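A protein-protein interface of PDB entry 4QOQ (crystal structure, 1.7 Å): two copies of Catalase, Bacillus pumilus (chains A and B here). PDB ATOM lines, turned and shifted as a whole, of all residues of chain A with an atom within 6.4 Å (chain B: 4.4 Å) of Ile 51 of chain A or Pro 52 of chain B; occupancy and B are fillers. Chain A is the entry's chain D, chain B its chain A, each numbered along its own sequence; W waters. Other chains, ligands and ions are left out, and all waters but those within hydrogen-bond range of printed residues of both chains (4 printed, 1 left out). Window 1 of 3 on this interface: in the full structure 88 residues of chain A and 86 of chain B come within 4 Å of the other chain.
A ring nitrogen (NE2) of His 346 of chain B sits at hydrogen-bond distance from the backbone carbonyl oxygen (O) of Arg 50 of chain A, at 3.1 Å.
The guanidinium group (NH1) of Arg 50 of chain A is in salt-bridge range of the side-chain carboxylate (OE2) of Glu 49 of chain A (2.9 Å).
Of the 6 printed residues of chain B, 3 touch a printed residue of chain A.
Among the printed residues, no Asp or Glu carboxylate lies within 4 Å of a Lys or Arg side-chain nitrogen of the other chain.
Printed residues of chain B within 4 Å of Arg 48 of chain A: His 346 (3.7 Å).
Printed residues of chain B within 4 Å of Arg 50 of chain A: Pro 52 (3.6 Å), Glu 53 (3.7 Å) and His 346 (3.1 Å).
Ile 51 of chain A touches just one residue of chain B: Pro 52 (3.98 Å).
Of the printed residues of chain B, Pro 52 of chain A touches Pro 52.
Glu 312 of chain A touches none of the printed residues of chain B.
Pro 52 of chain B touches just these residues of chain A: Arg 50 (3.6 Å), Ile 51 (3.98 Å) and Pro 52 (3.95 Å).
Printed residues of chain A within 4 Å of Glu 53 of chain B: Arg 50.
Printed residues of chain A within 4 Å of His 346 of chain B: Arg 48 (3.7 Å) and Arg 50 (3.1 Å).
The nearest printed residue of chain B that does not touch Ile 51 of chain A is Glu 53 of chain B (4.8 Å).
Water W4 lies within hydrogen-bond range of OE1 of Glu 53 of chain A (2.6 Å) and OE1 of Glu 53 of chain B (2.7 Å).
Water W2 bridges O of Ile 51 of chain B and N of Glu 53 of chain A.
Water W3 lies within hydrogen-bond range of the side-chain carboxylate of Glu 53 of chain B, the backbone carbonyl oxygen of Arg 54 of chain B and the guanidinium group of Arg 50 of chain A.
Water W1 bridges O of Ile 51 of chain A (2.8 Å) and N of Glu 53 of chain B (3.0 Å).
Arg 48 of chain A touches His 346 of chain B (CG to CG, 3.7 Å).
Pro 52 of chain B touches Arg 50 of chain A.
Arg 50 of chain A touches Glu 53 of chain B (CG to O, 3.7 Å).
Ile 51 of chain A touches Pro 52 of chain B.
Pro 52 of chain B touches Pro 52 of chain A (CA to N, 3.95 Å).
Ile 51 of chain A touches Pro 52 of chain B, but with the chains exchanged Pro 52 of chain A does not touch Ile 51 of chain B (4.02 Å).
Pro 52 of chain A touches its own counterpart, Pro 52 of chain B.
Positions printed for both chains: 51, 52, 53 and 347.
Of the 6 pairs that touch across the chains among the printed residues, 1 has its exchanged pair printed and touching as well.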
ATOM      1  N   ARG A  48      11.656  -9.374  -4.189  1.00  0.00           N
ATOM      2  CA  ARG A  48      11.508 -10.697  -4.746  1.00  0.00           C
ATOM      3  C   ARG A  48      11.747 -10.782  -6.266  1.00  0.00           C
ATOM      4  O   ARG A  48      11.356 -11.832  -6.877  1.00  0.00           O
ATOM      5  CB  ARG A  48      10.087 -11.244  -4.426  1.00  0.00           C
ATOM      6  CG  ARG A  48       9.941 -11.570  -2.957  1.00  0.00           C
ATOM      7  CD  ARG A  48       8.510 -11.890  -2.594  1.00  0.00           C
ATOM      8  NE  ARG A  48       8.537 -12.193  -1.157  1.00  0.00           N
ATOM      9  CZ  ARG A  48       8.755 -11.277  -0.188  1.00  0.00           C
ATOM     10  NH1 ARG A  48       8.653  -9.968  -0.406  1.00  0.00           N
ATOM     11  NH2 ARG A  48       8.935 -11.717   1.034  1.00  0.00           N
ATOM     12  N   GLU A  49      12.380  -9.764  -6.880  1.00  0.00           N
ATOM     13  CA  GLU A  49      12.661  -9.813  -8.292  1.00  0.00           C
ATOM     14  C   GLU A  49      13.545 -10.963  -8.752  1.00  0.00           C
ATOM     15  O   GLU A  49      13.324 -11.453  -9.873  1.00  0.00           O
ATOM     16  CB  GLU A  49      13.242  -8.506  -8.815  1.00  0.00           C
ATOM     17  CG  GLU A  49      12.251  -7.373  -8.778  1.00  0.00           C
ATOM     18  CD  GLU A  49      12.771  -6.044  -9.348  1.00  0.00           C
ATOM     19  OE1 GLU A  49      12.101  -5.037  -9.152  1.00  0.00           O
ATOM     20  OE2 GLU A  49      13.882  -6.007  -9.887  1.00  0.00           O
ATOM     21  N   ARG A  50      14.554 -11.331  -7.982  1.00  0.00           N
ATOM     22  CA  ARG A  50      15.566 -12.235  -8.429  1.00  0.00           C
ATOM     23  C   ARG A  50      15.187 -13.704  -8.258  1.00  0.00           C
ATOM     24  O   ARG A  50      14.604 -14.083  -7.229  1.00  0.00           O
ATOM     25  CB  ARG A  50      16.875 -11.975  -7.710  1.00  0.00           C
ATOM     26  CG  ARG A  50      17.392 -10.519  -7.830  1.00  0.00           C
ATOM     27  CD  ARG A  50      17.796 -10.097  -9.291  1.00  0.00           C
ATOM     28  NE  ARG A  50      18.100  -8.679  -9.225  1.00  0.00           N
ATOM     29  CZ  ARG A  50      17.297  -7.696  -9.577  1.00  0.00           C
ATOM     30  NH1 ARG A  50      16.130  -7.889 -10.186  1.00  0.00           N
ATOM     31  NH2 ARG A  50      17.675  -6.464  -9.317  1.00  0.00           N
ATOM     32  N   ILE A  51      15.603 -14.528  -9.226  1.00  0.00           N
ATOM     33  CA  ILE A  51      15.535 -15.964  -9.166  1.00  0.00           C
ATOM     34  C   ILE A  51      16.967 -16.499  -9.273  1.00  0.00           C
ATOM     35  O   ILE A  51      17.878 -15.767  -9.747  1.00  0.00           O
ATOM     36  CB  ILE A  51      14.552 -16.492 -10.270  1.00  0.00           C
ATOM     37  CG1 ILE A  51      15.125 -16.304 -11.648  1.00  0.00           C
ATOM     38  CG2 ILE A  51      13.185 -15.810 -10.107  1.00  0.00           C
ATOM     39  CD1 ILE A  51      14.349 -16.973 -12.737  1.00  0.00           C
ATOM     40  N   PRO A  52      17.219 -17.752  -8.855  1.00  0.00           N
ATOM     41  CA  PRO A  52      18.554 -18.350  -9.080  1.00  0.00           C
ATOM     42  C   PRO A  52      19.056 -18.231 -10.513  1.00  0.00           C
ATOM     43  O   PRO A  52      18.271 -18.394 -11.445  1.00  0.00           O
ATOM     44  CB  PRO A  52      18.379 -19.796  -8.691  1.00  0.00           C
ATOM     45  CG  PRO A  52      17.094 -19.866  -7.904  1.00  0.00           C
ATOM     46  CD  PRO A  52      16.212 -18.762  -8.478  1.00  0.00           C
ATOM     47  N   GLU A  53      20.334 -17.890 -10.679  1.00  0.00           N
ATOM     48  CA  GLU A  53      20.906 -17.896 -12.008  1.00  0.00           C
ATOM     49  C   GLU A  53      21.165 -19.362 -12.382  1.00  0.00           C
ATOM     50  O   GLU A  53      21.115 -20.263 -11.523  1.00  0.00           O
ATOM     51  CB  GLU A  53      22.214 -17.093 -12.117  1.00  0.00           C
ATOM     52  CG  GLU A  53      23.395 -17.708 -11.391  1.00  0.00           C
ATOM     53  CD  GLU A  53      24.691 -16.878 -11.493  1.00  0.00           C
ATOM     54  OE1 GLU A  53      24.604 -15.648 -11.725  1.00  0.00           O
ATOM     55  OE2 GLU A  53      25.788 -17.518 -11.313  1.00  0.00           O
ATOM     56  N   LYS A 102      26.207 -14.431 -13.754  1.00  0.00           N
ATOM     57  CA  LYS A 102      25.417 -13.631 -14.665  1.00  0.00           C
ATOM     58  C   LYS A 102      26.060 -12.394 -15.219  1.00  0.00           C
ATOM     59  O   LYS A 102      25.772 -12.026 -16.348  1.00  0.00           O
ATOM     60  CB  LYS A 102      24.175 -13.135 -13.942  1.00  0.00           C
ATOM     61  CG  LYS A 102      23.038 -13.997 -14.356  1.00  0.00           C
ATOM     62  CD  LYS A 102      21.738 -13.629 -13.642  1.00  0.00           C
ATOM     63  CE  LYS A 102      21.101 -12.289 -14.029  1.00  0.00           C
ATOM     64  NZ  LYS A 102      20.771 -12.166 -15.500  1.00  0.00           N
ATOM     65  N   PHE A 308      14.401 -10.444 -18.829  1.00  0.00           N
ATOM     66  CA  PHE A 308      14.088 -11.419 -17.747  1.00  0.00           C
ATOM     67  C   PHE A 308      13.082 -12.407 -18.186  1.00  0.00           C
ATOM     68  O   PHE A 308      13.296 -13.628 -17.972  1.00  0.00           O
ATOM     69  CB  PHE A 308      13.609 -10.751 -16.517  1.00  0.00           C
ATOM     70  CG  PHE A 308      13.262 -11.704 -15.419  1.00  0.00           C
ATOM     71  CD1 PHE A 308      14.241 -12.165 -14.545  1.00  0.00           C
ATOM     72  CD2 PHE A 308      11.957 -12.136 -15.249  1.00  0.00           C
ATOM     73  CE1 PHE A 308      13.922 -13.053 -13.509  1.00  0.00           C
ATOM     74  CE2 PHE A 308      11.624 -12.986 -14.247  1.00  0.00           C
ATOM     75  CZ  PHE A 308      12.616 -13.409 -13.342  1.00  0.00           C
ATOM     76  N   GLU A 312      16.144 -14.719 -19.619  1.00  0.00           N
ATOM     77  CA  GLU A 312      16.553 -15.285 -18.326  1.00  0.00           C
ATOM     78  C   GLU A 312      15.738 -16.506 -17.962  1.00  0.00           C
ATOM     79  O   GLU A 312      16.273 -17.439 -17.416  1.00  0.00           O
ATOM     80  CB  GLU A 312      16.509 -14.220 -17.211  1.00  0.00           C
ATOM     81  CG  GLU A 312      17.061 -14.733 -15.885  1.00  0.00           C
ATOM     82  CD  GLU A 312      18.576 -15.074 -15.907  1.00  0.00           C
ATOM     83  OE1 GLU A 312      19.066 -15.871 -15.053  1.00  0.00           O
ATOM     84  OE2 GLU A 312      19.321 -14.495 -16.664  1.00  0.00           O
ATOM     85  N   GLN A 313      14.419 -16.504 -18.270  1.00  0.00           N
ATOM     86  CA  GLN A 313      13.533 -17.618 -17.920  1.00  0.00           C
ATOM     87  C   GLN A 313      13.473 -18.728 -19.013  1.00  0.00           C
ATOM     88  O   GLN A 313      12.819 -19.691 -18.797  1.00  0.00           O
ATOM     89  CB  GLN A 313      12.143 -17.156 -17.698  1.00  0.00           C
ATOM     90  CG  GLN A 313      11.894 -16.329 -16.375  1.00  0.00           C
ATOM     91  CD  GLN A 313      10.409 -16.080 -16.054  1.00  0.00           C
ATOM     92  OE1 GLN A 313       9.925 -16.394 -14.970  1.00  0.00           O
ATOM     93  NE2 GLN A 313       9.679 -15.585 -17.012  1.00  0.00           N
ATOM     94  N   ARG A 347      14.939 -23.763 -10.660  1.00  0.00           N
ATOM     95  CA  ARG A 347      15.248 -22.365 -11.069  1.00  0.00           C
ATOM     96  C   ARG A 347      14.014 -21.522 -11.398  1.00  0.00           C
ATOM     97  O   ARG A 347      13.988 -20.376 -11.085  1.00  0.00           O
ATOM     98  CB  ARG A 347      16.190 -22.374 -12.262  1.00  0.00           C
ATOM     99  CG  ARG A 347      16.656 -21.048 -12.711  1.00  0.00           C
ATOM    100  CD  ARG A 347      17.805 -21.156 -13.686  1.00  0.00           C
ATOM    101  NE  ARG A 347      17.522 -21.711 -14.998  1.00  0.00           N
ATOM    102  CZ  ARG A 347      16.952 -21.056 -16.035  1.00  0.00           C
ATOM    103  NH1 ARG A 347      16.570 -19.760 -15.900  1.00  0.00           N
ATOM    104  NH2 ARG A 347      16.811 -21.673 -17.208  1.00  0.00           N
ATOM    105  N   LEU A 348      13.016 -22.134 -11.984  1.00  0.00           N
ATOM    106  CA  LEU A 348      11.900 -21.437 -12.583  1.00  0.00           C
ATOM    107  C   LEU A 348      10.536 -21.779 -12.032  1.00  0.00           C
ATOM    108  O   LEU A 348       9.574 -21.053 -12.251  1.00  0.00           O
ATOM    109  CB  LEU A 348      11.938 -21.729 -14.087  1.00  0.00           C
ATOM    110  CG  LEU A 348      13.128 -21.193 -14.917  1.00  0.00           C
ATOM    111  CD1 LEU A 348      13.135 -21.858 -16.283  1.00  0.00           C
ATOM    112  CD2 LEU A 348      13.145 -19.664 -14.937  1.00  0.00           C
ATOM    113  N   ILE B  51      21.142 -20.056  -5.313  1.00  0.00           N
ATOM    114  CA  ILE B  51      20.021 -19.291  -4.711  1.00  0.00           C
ATOM    115  C   ILE B  51      19.991 -17.853  -5.362  1.00  0.00           C
ATOM    116  O   ILE B  51      21.001 -17.417  -5.984  1.00  0.00           O
ATOM    117  CB  ILE B  51      20.177 -19.241  -3.165  1.00  0.00           C
ATOM    118  CG1 ILE B  51      21.341 -18.313  -2.754  1.00  0.00           C
ATOM    119  CG2 ILE B  51      20.319 -20.651  -2.643  1.00  0.00           C
ATOM    120  CD1 ILE B  51      21.421 -18.115  -1.268  1.00  0.00           C
ATOM    121  N   PRO B  52      18.879 -17.153  -5.264  1.00  0.00           N
ATOM    122  CA  PRO B  52      18.831 -15.779  -5.834  1.00  0.00           C
ATOM    123  C   PRO B  52      19.924 -14.881  -5.287  1.00  0.00           C
ATOM    124  O   PRO B  52      20.267 -14.990  -4.159  1.00  0.00           O
ATOM    125  CB  PRO B  52      17.465 -15.262  -5.381  1.00  0.00           C
ATOM    126  CG  PRO B  52      16.663 -16.454  -5.061  1.00  0.00           C
ATOM    127  CD  PRO B  52      17.648 -17.461  -4.503  1.00  0.00           C
ATOM    128  N   GLU B  53      20.524 -14.062  -6.157  1.00  0.00           N
ATOM    129  CA  GLU B  53      21.547 -13.135  -5.723  1.00  0.00           C
ATOM    130  C   GLU B  53      20.813 -11.945  -5.052  1.00  0.00           C
ATOM    131  O   GLU B  53      19.595 -11.838  -5.156  1.00  0.00           O
ATOM    132  CB  GLU B  53      22.448 -12.657  -6.850  1.00  0.00           C
ATOM    133  CG  GLU B  53      21.753 -11.729  -7.822  1.00  0.00           C
ATOM    134  CD  GLU B  53      22.678 -11.236  -8.938  1.00  0.00           C
ATOM    135  OE1 GLU B  53      23.713 -11.892  -9.278  1.00  0.00           O
ATOM    136  OE2 GLU B  53      22.292 -10.181  -9.620  1.00  0.00           O
ATOM    137  N   ARG B  54      21.538 -11.173  -4.280  1.00  0.00           N
ATOM    138  CA  ARG B  54      20.906  -9.974  -3.643  1.00  0.00           C
ATOM    139  C   ARG B  54      20.381  -9.060  -4.727  1.00  0.00           C
ATOM    140  O   ARG B  54      21.022  -8.872  -5.766  1.00  0.00           O
ATOM    141  CB  ARG B  54      21.965  -9.227  -2.844  1.00  0.00           C
ATOM    142  CG  ARG B  54      22.508  -9.966  -1.608  1.00  0.00           C
ATOM    143  CD  ARG B  54      23.794  -9.352  -1.182  1.00  0.00           C
ATOM    144  NE  ARG B  54      24.283  -9.947   0.079  1.00  0.00           N
ATOM    145  CZ  ARG B  54      24.844 -11.136   0.198  1.00  0.00           C
ATOM    146  NH1 ARG B  54      24.934 -11.947  -0.846  1.00  0.00           N
ATOM    147  NH2 ARG B  54      25.226 -11.597   1.400  1.00  0.00           N
ATOM    148  N   HIS B 346      12.884 -14.336   1.464  1.00  0.00           N
ATOM    149  CA  HIS B 346      12.886 -14.822   0.095  1.00  0.00           C
ATOM    150  C   HIS B 346      14.194 -15.404  -0.369  1.00  0.00           C
ATOM    151  O   HIS B 346      14.218 -16.576  -0.901  1.00  0.00           O
ATOM    152  CB  HIS B 346      12.428 -13.672  -0.859  1.00  0.00           C
ATOM    153  CG  HIS B 346      12.767 -13.892  -2.301  1.00  0.00           C
ATOM    154  ND1 HIS B 346      12.129 -14.831  -3.087  1.00  0.00           N
ATOM    155  CD2 HIS B 346      13.676 -13.300  -3.088  1.00  0.00           C
ATOM    156  CE1 HIS B 346      12.617 -14.791  -4.307  1.00  0.00           C
ATOM    157  NE2 HIS B 346      13.596 -13.900  -4.332  1.00  0.00           N
ATOM    158  N   ARG B 347      15.276 -14.619  -0.227  1.00  0.00           N
ATOM    159  CA  ARG B 347      16.572 -15.014  -0.758  1.00  0.00           C
ATOM    160  C   ARG B 347      17.150 -16.265  -0.091  1.00  0.00           C
ATOM    161  O   ARG B 347      17.803 -17.082  -0.698  1.00  0.00           O
ATOM    162  CB  ARG B 347      17.522 -13.858  -0.624  1.00  0.00           C
ATOM    163  CG  ARG B 347      18.897 -14.088  -1.184  1.00  0.00           C
ATOM    164  CD  ARG B 347      19.701 -12.869  -1.292  1.00  0.00           C
ATOM    165  NE  ARG B 347      20.129 -12.256  -0.019  1.00  0.00           N
ATOM    166  CZ  ARG B 347      21.197 -12.606   0.687  1.00  0.00           C
ATOM    167  NH1 ARG B 347      21.948 -13.681   0.344  1.00  0.00           N
ATOM    168  NH2 ARG B 347      21.484 -11.884   1.776  1.00  0.00           N
HETATM  169  O   HOH W   1      20.083 -14.258  -9.094  1.00  0.00           O
HETATM  170  O   HOH W   2      21.934 -16.909  -8.436  1.00  0.00           O
HETATM  171  O   HOH W   3      20.905  -8.200  -8.434  1.00  0.00           O
HETATM  172  O   HOH W   4      23.107 -14.492  -9.925  1.00  0.00           O
